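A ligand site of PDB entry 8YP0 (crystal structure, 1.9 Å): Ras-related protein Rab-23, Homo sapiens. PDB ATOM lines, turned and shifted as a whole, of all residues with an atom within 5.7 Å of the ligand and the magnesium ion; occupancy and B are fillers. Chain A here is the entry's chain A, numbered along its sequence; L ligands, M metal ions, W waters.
Residues that only touch the ligand: Asn 12 (3.9 Å), Gly 13 (3.4 Å), Phe 29 (3.4 Å), Gly 62 (3.7 Å), Leu 119 (3.6 Å) and Ser 145 (3.5 Å).
The nearest printed residue that does not touch the ligand is Thr 30 (4.5 Å).
Water W11 bridges O of Lys 35 (2.7 Å) and O8 of the ligand (2.8 Å).
Water W7 bridges O of Thr 60 (2.8 Å) and OD1 of Asp 59 (2.8 Å).
Water W3 bridges an oxygen (O11) of the ligand and the backbone carbonyl oxygen (O) of Asp 32.
Water W8 lies within hydrogen-bond range of N of Lys 35, O of Tyr 33 and O8 of the ligand.
Water W13 lies within hydrogen-bond range of NZ of Lys 116 and N6 of the ligand.
Asp 59 touches the magnesium ion.
Within 4 Å of the magnesium ion: Ser 18 and Asp 59.
Along chain A the residues within 4 Å of the magnesium ion span positions 18 to 59.
The magnesium ion is bound by water W7 (2.0 Å), water W11 (2.0 Å), an oxygen (O1) of the ligand (2.1 Å), the side-chain hydroxyl (OG) of Ser 18 (2.2 Å), water W2 (2.2 Å) and an oxygen (O5) of the ligand (2.2 Å).
N of Ser 18 lies within hydrogen-bond range of O7 of the ligand (3.5 Å).
The backbone NH (N) of Lys 17 lies within hydrogen-bond range of an oxygen (O4) of the ligand.
An oxygen (O4) of the ligand is in salt-bridge range of the side-chain amino group (NZ) of Lys 17.
The backbone NH of Val 146 is in hydrogen-bond range of an oxygen (O13) of the ligand (2.8 Å).
An oxygen (O7) of the ligand sits at hydrogen-bond distance from the backbone NH (N) of Ser 19, at 2.8 Å.
OG of Ser 19 sits at hydrogen-bond distance from O7 of the ligand (2.8 Å).
The side-chain carboxylate of Asp 118 is in hydrogen-bond range of a nitrogen (N5) of the ligand, at 2.8 Å.
The side-chain amino group of Lys 35 is in hydrogen-bond range of an oxygen (O12) of the ligand, at 2.9 Å.
The backbone NH (N) of Ala 14 sits at hydrogen-bond distance from an oxygen (O4) of the ligand, at 3.5 Å.
The side-chain amino group (NZ) of Lys 116 lies within hydrogen-bond range of an oxygen (O10) of the ligand, 3.1 Å away.
ND2 of Asn 115 lies within hydrogen-bond range of N3 of the ligand.
N of Lys 147 is in hydrogen-bond range of O13 of the ligand.
The backbone NH (N) of Gly 16 sits at hydrogen-bond distance from an oxygen (O4) of the ligand, 3.2 Å away.
O4 of the ligand lies within hydrogen-bond range of N of Val 15 (3.4 Å).
OD2 of Asp 59 lies close to OG of Ser 18, at 2.5 Å.
NZ of Lys 35 sits close to OG of Ser 19.
OG of Ser 145 lies within hydrogen-bond range of OD1 of Asp 118.
The backbone carbonyl oxygen (O) of Ala 14 sits at hydrogen-bond distance from the side-chain amino group (NZ) of Lys 116, 2.8 Å away.
N of Lys 116 lies within hydrogen-bond range of O of Thr 144 (3.1 Å).
The backbone carbonyl oxygen (O) of Val 15 sits at hydrogen-bond distance from the side-chain amide nitrogen (ND2) of Asn 115.
OG1 of Thr 144 lies within hydrogen-bond range of OD1 of Asn 115.
The side-chain hydroxyl of Ser 145 sits at hydrogen-bond distance from the backbone NH of Glu 148 (3.2 Å).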
ATOM      1  N   GLY A  11      24.841  -1.954  -0.235  1.00  0.00           N
ATOM      2  CA  GLY A  11      24.337  -1.924   1.128  1.00  0.00           C
ATOM      3  C   GLY A  11      23.087  -2.768   1.271  1.00  0.00           C
ATOM      4  O   GLY A  11      22.502  -3.233   0.297  1.00  0.00           O
ATOM      5  N   ASN A  12      22.668  -2.947   2.531  1.00  0.00           N
ATOM      6  CA  ASN A  12      21.512  -3.784   2.848  1.00  0.00           C
ATOM      7  C   ASN A  12      20.231  -3.199   2.243  1.00  0.00           C
ATOM      8  O   ASN A  12      20.177  -2.055   1.798  1.00  0.00           O
ATOM      9  CB  ASN A  12      21.356  -3.945   4.357  1.00  0.00           C
ATOM     10  CG  ASN A  12      22.161  -5.112   4.909  1.00  0.00           C
ATOM     11  OD1 ASN A  12      23.161  -5.525   4.328  1.00  0.00           O
ATOM     12  ND2 ASN A  12      21.719  -5.638   6.044  1.00  0.00           N
ATOM     13  N   GLY A  13      19.181  -4.023   2.250  1.00  0.00           N
ATOM     14  CA  GLY A  13      17.916  -3.596   1.678  1.00  0.00           C
ATOM     15  C   GLY A  13      17.351  -2.387   2.402  1.00  0.00           C
ATOM     16  O   GLY A  13      17.485  -2.244   3.616  1.00  0.00           O
ATOM     17  N   ALA A  14      16.775  -1.468   1.621  1.00  0.00           N
ATOM     18  CA  ALA A  14      16.024  -0.307   2.086  1.00  0.00           C
ATOM     19  C   ALA A  14      16.904   0.774   2.722  1.00  0.00           C
ATOM     20  O   ALA A  14      16.389   1.718   3.332  1.00  0.00           O
ATOM     21  CB  ALA A  14      14.921  -0.699   3.075  1.00  0.00           C
ATOM     22  N   VAL A  15      18.235   0.697   2.576  1.00  0.00           N
ATOM     23  CA  VAL A  15      19.079   1.748   3.141  1.00  0.00           C
ATOM     24  C   VAL A  15      19.031   3.015   2.305  1.00  0.00           C
ATOM     25  O   VAL A  15      19.439   4.076   2.790  1.00  0.00           O
ATOM     26  CB  VAL A  15      20.539   1.286   3.290  1.00  0.00           C
ATOM     27  CG1 VAL A  15      20.646   0.086   4.223  1.00  0.00           C
ATOM     28  CG2 VAL A  15      21.152   1.000   1.935  1.00  0.00           C
ATOM     29  N   GLY A  16      18.563   2.952   1.066  1.00  0.00           N
ATOM     30  CA  GLY A  16      18.415   4.124   0.232  1.00  0.00           C
ATOM     31  C   GLY A  16      19.266   4.143  -1.037  1.00  0.00           C
ATOM     32  O   GLY A  16      19.455   5.223  -1.610  1.00  0.00           O
ATOM     33  N   LYS A  17      19.745   2.992  -1.513  1.00  0.00           N
ATOM     34  CA  LYS A  17      20.644   2.957  -2.663  1.00  0.00           C
ATOM     35  C   LYS A  17      19.979   3.543  -3.913  1.00  0.00           C
ATOM     36  O   LYS A  17      20.531   4.448  -4.553  1.00  0.00           O
ATOM     37  CB  LYS A  17      21.103   1.515  -2.920  1.00  0.00           C
ATOM     38  CG  LYS A  17      21.800   0.868  -1.728  1.00  0.00           C
ATOM     39  CD  LYS A  17      22.299  -0.543  -2.057  1.00  0.00           C
ATOM     40  CE  LYS A  17      21.150  -1.522  -2.284  1.00  0.00           C
ATOM     41  NZ  LYS A  17      20.304  -1.707  -1.067  1.00  0.00           N
ATOM     42  N   SER A  18      18.805   3.037  -4.273  1.00  0.00           N
ATOM     43  CA  SER A  18      18.127   3.514  -5.473  1.00  0.00           C
ATOM     44  C   SER A  18      17.766   4.990  -5.357  1.00  0.00           C
ATOM     45  O   SER A  18      17.919   5.751  -6.313  1.00  0.00           O
ATOM     46  CB  SER A  18      16.878   2.681  -5.735  1.00  0.00           C
ATOM     47  OG  SER A  18      17.197   1.304  -5.931  1.00  0.00           O
ATOM     48  N   SER A  19      17.281   5.404  -4.176  1.00  0.00           N
ATOM     49  CA  SER A  19      16.957   6.812  -3.954  1.00  0.00           C
ATOM     50  C   SER A  19      18.186   7.696  -4.058  1.00  0.00           C
ATOM     51  O   SER A  19      18.111   8.810  -4.601  1.00  0.00           O
ATOM     52  CB  SER A  19      16.303   6.983  -2.578  1.00  0.00           C
ATOM     53  OG  SER A  19      15.054   6.336  -2.506  1.00  0.00           O
ATOM     54  N   MET A  20      19.322   7.236  -3.538  1.00  0.00           N
ATOM     55  CA  MET A  20      20.551   8.019  -3.635  1.00  0.00           C
ATOM     56  C   MET A  20      20.930   8.259  -5.079  1.00  0.00           C
ATOM     57  O   MET A  20      21.294   9.378  -5.464  1.00  0.00           O
ATOM     58  CB  MET A  20      21.691   7.311  -2.899  1.00  0.00           C
ATOM     59  CG  MET A  20      22.953   8.134  -2.813  1.00  0.00           C
ATOM     60  SD  MET A  20      24.254   7.315  -1.857  1.00  0.00           S
ATOM     61  CE  MET A  20      23.474   7.189  -0.259  1.00  0.00           C
ATOM     62  N   PHE A  29      13.210  13.047  -5.438  1.00  0.00           N
ATOM     63  CA  PHE A  29      12.993  12.116  -4.330  1.00  0.00           C
ATOM     64  C   PHE A  29      11.493  11.865  -4.302  1.00  0.00           C
ATOM     65  O   PHE A  29      10.724  12.711  -3.822  1.00  0.00           O
ATOM     66  CB  PHE A  29      13.505  12.679  -3.004  1.00  0.00           C
ATOM     67  CG  PHE A  29      13.261  11.779  -1.835  1.00  0.00           C
ATOM     68  CD1 PHE A  29      14.121  10.721  -1.552  1.00  0.00           C
ATOM     69  CD2 PHE A  29      12.171  11.986  -0.988  1.00  0.00           C
ATOM     70  CE1 PHE A  29      13.897   9.888  -0.472  1.00  0.00           C
ATOM     71  CE2 PHE A  29      11.948  11.153   0.092  1.00  0.00           C
ATOM     72  CZ  PHE A  29      12.807  10.104   0.360  1.00  0.00           C
ATOM     73  N   THR A  30      11.076  10.729  -4.832  1.00  0.00           N
ATOM     74  CA  THR A  30       9.656  10.453  -5.026  1.00  0.00           C
ATOM     75  C   THR A  30       9.053   9.788  -3.794  1.00  0.00           C
ATOM     76  O   THR A  30       9.753   9.269  -2.924  1.00  0.00           O
ATOM     77  CB  THR A  30       9.447   9.568  -6.247  1.00  0.00           C
ATOM     78  OG1 THR A  30      10.189   8.363  -6.086  1.00  0.00           O
ATOM     79  CG2 THR A  30       9.908  10.281  -7.509  1.00  0.00           C
ATOM     80  N   ASP A  32       7.462   7.166  -4.239  1.00  0.00           N
ATOM     81  CA  ASP A  32       7.239   5.850  -4.842  1.00  0.00           C
ATOM     82  C   ASP A  32       7.311   4.766  -3.777  1.00  0.00           C
ATOM     83  O   ASP A  32       8.105   4.843  -2.846  1.00  0.00           O
ATOM     84  CB  ASP A  32       8.285   5.588  -5.928  1.00  0.00           C
ATOM     85  CG  ASP A  32       7.659   5.311  -7.279  1.00  0.00           C
ATOM     86  OD1 ASP A  32       7.139   6.261  -7.897  1.00  0.00           O
ATOM     87  OD2 ASP A  32       7.703   4.147  -7.734  1.00  0.00           O
ATOM     88  N   TYR A  33       6.458   3.756  -3.927  1.00  0.00           N
ATOM     89  CA  TYR A  33       6.427   2.660  -2.956  1.00  0.00           C
ATOM     90  C   TYR A  33       7.603   1.715  -3.145  1.00  0.00           C
ATOM     91  O   TYR A  33       8.368   1.464  -2.199  1.00  0.00           O
ATOM     92  CB  TYR A  33       5.098   1.907  -3.064  1.00  0.00           C
ATOM     93  N   LYS A  35      10.673   1.761  -5.188  1.00  0.00           N
ATOM     94  CA  LYS A  35      11.542   2.545  -6.043  1.00  0.00           C
ATOM     95  C   LYS A  35      12.484   1.641  -6.825  1.00  0.00           C
ATOM     96  O   LYS A  35      13.151   0.770  -6.250  1.00  0.00           O
ATOM     97  CB  LYS A  35      12.335   3.556  -5.228  1.00  0.00           C
ATOM     98  CG  LYS A  35      11.475   4.483  -4.417  1.00  0.00           C
ATOM     99  CD  LYS A  35      12.241   5.679  -3.921  1.00  0.00           C
ATOM    100  CE  LYS A  35      11.333   6.589  -3.117  1.00  0.00           C
ATOM    101  NZ  LYS A  35      12.072   7.781  -2.622  1.00  0.00           N
ATOM    102  N   ASP A  59      23.238   0.659  -9.657  1.00  0.00           N
ATOM    103  CA  ASP A  59      22.423   0.187  -8.545  1.00  0.00           C
ATOM    104  C   ASP A  59      22.650  -1.314  -8.324  1.00  0.00           C
ATOM    105  O   ASP A  59      23.018  -2.039  -9.246  1.00  0.00           O
ATOM    106  CB  ASP A  59      20.944   0.461  -8.845  1.00  0.00           C
ATOM    107  CG  ASP A  59      20.092   0.593  -7.593  1.00  0.00           C
ATOM    108  OD1 ASP A  59      20.634   0.515  -6.476  1.00  0.00           O
ATOM    109  OD2 ASP A  59      18.865   0.785  -7.736  1.00  0.00           O
ATOM    110  N   THR A  60      22.422  -1.760  -7.088  1.00  0.00           N
ATOM    111  CA  THR A  60      22.588  -3.168  -6.720  1.00  0.00           C
ATOM    112  C   THR A  60      21.410  -3.611  -5.858  1.00  0.00           C
ATOM    113  O   THR A  60      20.612  -2.802  -5.397  1.00  0.00           O
ATOM    114  CB  THR A  60      23.903  -3.431  -5.952  1.00  0.00           C
ATOM    115  OG1 THR A  60      23.883  -2.691  -4.721  1.00  0.00           O
ATOM    116  CG2 THR A  60      25.114  -3.020  -6.768  1.00  0.00           C
ATOM    117  N   ALA A  61      21.330  -4.923  -5.626  1.00  0.00           N
ATOM    118  CA  ALA A  61      20.322  -5.503  -4.755  1.00  0.00           C
ATOM    119  C   ALA A  61      20.870  -5.668  -3.333  1.00  0.00           C
ATOM    120  O   ALA A  61      22.086  -5.756  -3.121  1.00  0.00           O
ATOM    121  CB  ALA A  61      19.845  -6.852  -5.293  1.00  0.00           C
ATOM    122  N   GLY A  62      19.960  -5.720  -2.376  1.00  0.00           N
ATOM    123  CA  GLY A  62      20.331  -5.903  -0.981  1.00  0.00           C
ATOM    124  C   GLY A  62      20.702  -7.333  -0.646  1.00  0.00           C
ATOM    125  O   GLY A  62      21.097  -7.624   0.488  1.00  0.00           O
ATOM    126  N   ASN A 115      22.988   6.948   5.770  1.00  0.00           N
ATOM    127  CA  ASN A 115      21.866   7.617   5.151  1.00  0.00           C
ATOM    128  C   ASN A 115      20.706   7.744   6.150  1.00  0.00           C
ATOM    129  O   ASN A 115      20.717   7.159   7.235  1.00  0.00           O
ATOM    130  CB  ASN A 115      21.425   6.858   3.898  1.00  0.00           C
ATOM    131  CG  ASN A 115      20.427   7.640   3.069  1.00  0.00           C
ATOM    132  OD1 ASN A 115      20.510   8.870   2.949  1.00  0.00           O
ATOM    133  ND2 ASN A 115      19.459   6.936   2.503  1.00  0.00           N
ATOM    134  N   LYS A 116      19.715   8.551   5.767  1.00  0.00           N
ATOM    135  CA  LYS A 116      18.501   8.785   6.544  1.00  0.00           C
ATOM    136  C   LYS A 116      18.787   9.525   7.849  1.00  0.00           C
ATOM    137  O   LYS A 116      18.106   9.319   8.861  1.00  0.00           O
ATOM    138  CB  LYS A 116      17.747   7.477   6.809  1.00  0.00           C
ATOM    139  CG  LYS A 116      17.465   6.660   5.558  1.00  0.00           C
ATOM    140  CD  LYS A 116      16.442   5.566   5.834  1.00  0.00           C
ATOM    141  CE  LYS A 116      16.224   4.700   4.604  1.00  0.00           C
ATOM    142  NZ  LYS A 116      15.178   3.671   4.845  1.00  0.00           N
ATOM    143  N   ILE A 117      19.786  10.401   7.823  1.00  0.00           N
ATOM    144  CA  ILE A 117      20.134  11.173   9.022  1.00  0.00           C
ATOM    145  C   ILE A 117      18.991  12.090   9.448  1.00  0.00           C
ATOM    146  O   ILE A 117      18.941  12.516  10.608  1.00  0.00           O
ATOM    147  CB  ILE A 117      21.436  11.966   8.785  1.00  0.00           C
ATOM    148  CG1 ILE A 117      22.127  12.291  10.106  1.00  0.00           C
ATOM    149  CG2 ILE A 117      21.175  13.224   7.970  1.00  0.00           C
ATOM    150  CD1 ILE A 117      22.548  11.075  10.888  1.00  0.00           C
ATOM    151  N   ASP A 118      18.035  12.366   8.550  1.00  0.00           N
ATOM    152  CA  ASP A 118      16.846  13.121   8.929  1.00  0.00           C
ATOM    153  C   ASP A 118      15.950  12.353   9.903  1.00  0.00           C
ATOM    154  O   ASP A 118      15.046  12.943  10.495  1.00  0.00           O
ATOM    155  CB  ASP A 118      16.034  13.494   7.682  1.00  0.00           C
ATOM    156  CG  ASP A 118      15.665  12.280   6.847  1.00  0.00           C
ATOM    157  OD1 ASP A 118      16.561  11.714   6.189  1.00  0.00           O
ATOM    158  OD2 ASP A 118      14.475  11.872   6.869  1.00  0.00           O
ATOM    159  N   LEU A 119      16.170  11.050  10.074  1.00  0.00           N
ATOM    160  CA  LEU A 119      15.426  10.232  11.028  1.00  0.00           C
ATOM    161  C   LEU A 119      16.214  10.010  12.306  1.00  0.00           C
ATOM    162  O   LEU A 119      16.081   8.976  12.956  1.00  0.00           O
ATOM    163  CB  LEU A 119      15.049   8.891  10.393  1.00  0.00           C
ATOM    164  CG  LEU A 119      14.181   8.929   9.132  1.00  0.00           C
ATOM    165  CD1 LEU A 119      13.949   7.516   8.600  1.00  0.00           C
ATOM    166  CD2 LEU A 119      12.859   9.635   9.397  1.00  0.00           C
ATOM    167  N   THR A 144      24.399  11.414   5.475  1.00  0.00           N
ATOM    168  CA  THR A 144      23.598  11.973   4.400  1.00  0.00           C
ATOM    169  C   THR A 144      22.114  11.805   4.685  1.00  0.00           C
ATOM    170  O   THR A 144      21.691  10.962   5.482  1.00  0.00           O
ATOM    171  CB  THR A 144      23.921  11.330   3.045  1.00  0.00           C
ATOM    172  OG1 THR A 144      23.377  10.008   2.992  1.00  0.00           O
ATOM    173  CG2 THR A 144      25.431  11.272   2.812  1.00  0.00           C
ATOM    174  N   SER A 145      21.324  12.651   4.022  1.00  0.00           N
ATOM    175  CA  SER A 145      19.868  12.499   3.931  1.00  0.00           C
ATOM    176  C   SER A 145      19.533  12.641   2.455  1.00  0.00           C
ATOM    177  O   SER A 145      19.536  13.757   1.922  1.00  0.00           O
ATOM    178  CB  SER A 145      19.141  13.530   4.776  1.00  0.00           C
ATOM    179  OG  SER A 145      17.738  13.429   4.584  1.00  0.00           O
ATOM    180  N   VAL A 146      19.252  11.525   1.794  1.00  0.00           N
ATOM    181  CA  VAL A 146      18.800  11.575   0.405  1.00  0.00           C
ATOM    182  C   VAL A 146      17.503  12.370   0.324  1.00  0.00           C
ATOM    183  O   VAL A 146      17.305  13.172  -0.605  1.00  0.00           O
ATOM    184  CB  VAL A 146      18.641  10.159  -0.167  1.00  0.00           C
ATOM    185  CG1 VAL A 146      18.010  10.213  -1.555  1.00  0.00           C
ATOM    186  CG2 VAL A 146      19.981   9.441  -0.224  1.00  0.00           C
ATOM    187  N   LYS A 147      16.620  12.181   1.299  1.00  0.00           N
ATOM    188  CA  LYS A 147      15.323  12.861   1.297  1.00  0.00           C
ATOM    189  C   LYS A 147      15.476  14.372   1.273  1.00  0.00           C
ATOM    190  O   LYS A 147      14.738  15.070   0.566  1.00  0.00           O
ATOM    191  CB  LYS A 147      14.515  12.418   2.519  1.00  0.00           C
ATOM    192  CG  LYS A 147      13.185  13.148   2.704  1.00  0.00           C
ATOM    193  CD  LYS A 147      12.383  12.538   3.847  1.00  0.00           C
ATOM    194  CE  LYS A 147      11.038  13.223   4.013  1.00  0.00           C
ATOM    195  NZ  LYS A 147      10.239  12.599   5.099  1.00  0.00           N
ATOM    196  N   GLU A 148      16.444  14.898   2.029  1.00  0.00           N
ATOM    197  CA  GLU A 148      16.632  16.343   2.139  1.00  0.00           C
ATOM    198  C   GLU A 148      17.798  16.858   1.300  1.00  0.00           C
ATOM    199  O   GLU A 148      18.134  18.039   1.384  1.00  0.00           O
ATOM    200  CB  GLU A 148      16.825  16.717   3.609  1.00  0.00           C
ATOM    201  CG  GLU A 148      15.605  16.410   4.481  1.00  0.00           C
ATOM    202  CD  GLU A 148      15.840  16.648   5.955  1.00  0.00           C
ATOM    203  OE1 GLU A 148      16.979  16.999   6.339  1.00  0.00           O
ATOM    204  OE2 GLU A 148      14.886  16.486   6.741  1.00  0.00           O
HETATM  205  P1  LIG L   1      16.500  -2.308  -2.082  1.00  0.00           P
HETATM  206  O1  LIG L   1      16.612  -2.149  -3.536  1.00  0.00           O
HETATM  207  O2  LIG L   1      17.792  -2.842  -1.622  1.00  0.00           O
HETATM  208  O3  LIG L   1      15.356  -3.146  -1.666  1.00  0.00           O
HETATM  209  N1  LIG L   1      16.355  -0.853  -1.332  1.00  0.00           N
HETATM  210  P2  LIG L   1      17.273   0.490  -1.466  1.00  0.00           P
HETATM  211  O4  LIG L   1      18.552   0.328  -0.756  1.00  0.00           O
HETATM  212  O5  LIG L   1      17.476   0.848  -2.881  1.00  0.00           O
HETATM  213  O6  LIG L   1      16.342   1.685  -0.867  1.00  0.00           O
HETATM  214  P3  LIG L   1      15.297   2.696  -1.522  1.00  0.00           P
HETATM  215  O7  LIG L   1      16.030   3.709  -2.299  1.00  0.00           O
HETATM  216  O8  LIG L   1      14.232   1.900  -2.185  1.00  0.00           O
HETATM  217  O9  LIG L   1      14.714   3.409  -0.217  1.00  0.00           O
HETATM  218  C1  LIG L   1      13.943   2.669   0.758  1.00  0.00           C
HETATM  219  C2  LIG L   1      12.997   3.616   1.452  1.00  0.00           C
HETATM  220  O10 LIG L   1      13.747   4.588   2.232  1.00  0.00           O
HETATM  221  C3  LIG L   1      12.104   4.426   0.518  1.00  0.00           C
HETATM  222  O11 LIG L   1      10.800   4.588   1.063  1.00  0.00           O
HETATM  223  C4  LIG L   1      12.836   5.763   0.407  1.00  0.00           C
HETATM  224  O12 LIG L   1      11.951   6.845   0.100  1.00  0.00           O
HETATM  225  C5  LIG L   1      13.387   5.903   1.828  1.00  0.00           C
HETATM  226  N2  LIG L   1      14.571   6.766   1.937  1.00  0.00           N
HETATM  227  C6  LIG L   1      15.698   6.772   1.161  1.00  0.00           C
HETATM  228  N3  LIG L   1      16.575   7.681   1.532  1.00  0.00           N
HETATM  229  C7  LIG L   1      15.982   8.304   2.615  1.00  0.00           C
HETATM  230  C8  LIG L   1      16.444   9.379   3.449  1.00  0.00           C
HETATM  231  O13 LIG L   1      17.505   9.997   3.365  1.00  0.00           O
HETATM  232  N4  LIG L   1      15.521   9.693   4.437  1.00  0.00           N
HETATM  233  C9  LIG L   1      14.315   9.071   4.615  1.00  0.00           C
HETATM  234  N5  LIG L   1      13.550   9.521   5.620  1.00  0.00           N
HETATM  235  N6  LIG L   1      13.883   8.077   3.848  1.00  0.00           N
HETATM  236  C10 LIG L   1      14.751   7.746   2.874  1.00  0.00           C
HETATM  237 MG    MG M   1      16.809  -0.335  -4.594  1.00  0.00          MG
HETATM  238  O   HOH W   1      13.437  -3.017  -4.084  1.00  0.00           O
HETATM  239  O   HOH W   2      16.267  -1.375  -6.412  1.00  0.00           O
HETATM  240  O   HOH W   3       8.850   5.093  -0.354  1.00  0.00           O
HETATM  241  O   HOH W   4       9.779   7.784   1.218  1.00  0.00           O
HETATM  242  O   HOH W   5      13.402  -0.780  -0.350  1.00  0.00           O
HETATM  243  O   HOH W   6      16.546  -4.290  -4.897  1.00  0.00           O
HETATM  244  O   HOH W   7      18.695  -0.832  -4.946  1.00  0.00           O
HETATM  245  O   HOH W   8      11.205   1.102  -2.498  1.00  0.00           O
HETATM  246  O   HOH W   9      10.390   8.587   5.766  1.00  0.00           O
HETATM  247  O   HOH W  10      13.990  -3.847   0.563  1.00  0.00           O
HETATM  248  O   HOH W  11      14.877   0.242  -4.300  1.00  0.00           O
HETATM  249  O   HOH W  12      10.748   4.293   4.069  1.00  0.00           O
HETATM  250  O   HOH W  13      12.661   5.366   5.515  1.00  0.00           O
HETATM  251  O   HOH W  14      11.686   0.350   1.991  1.00  0.00           O
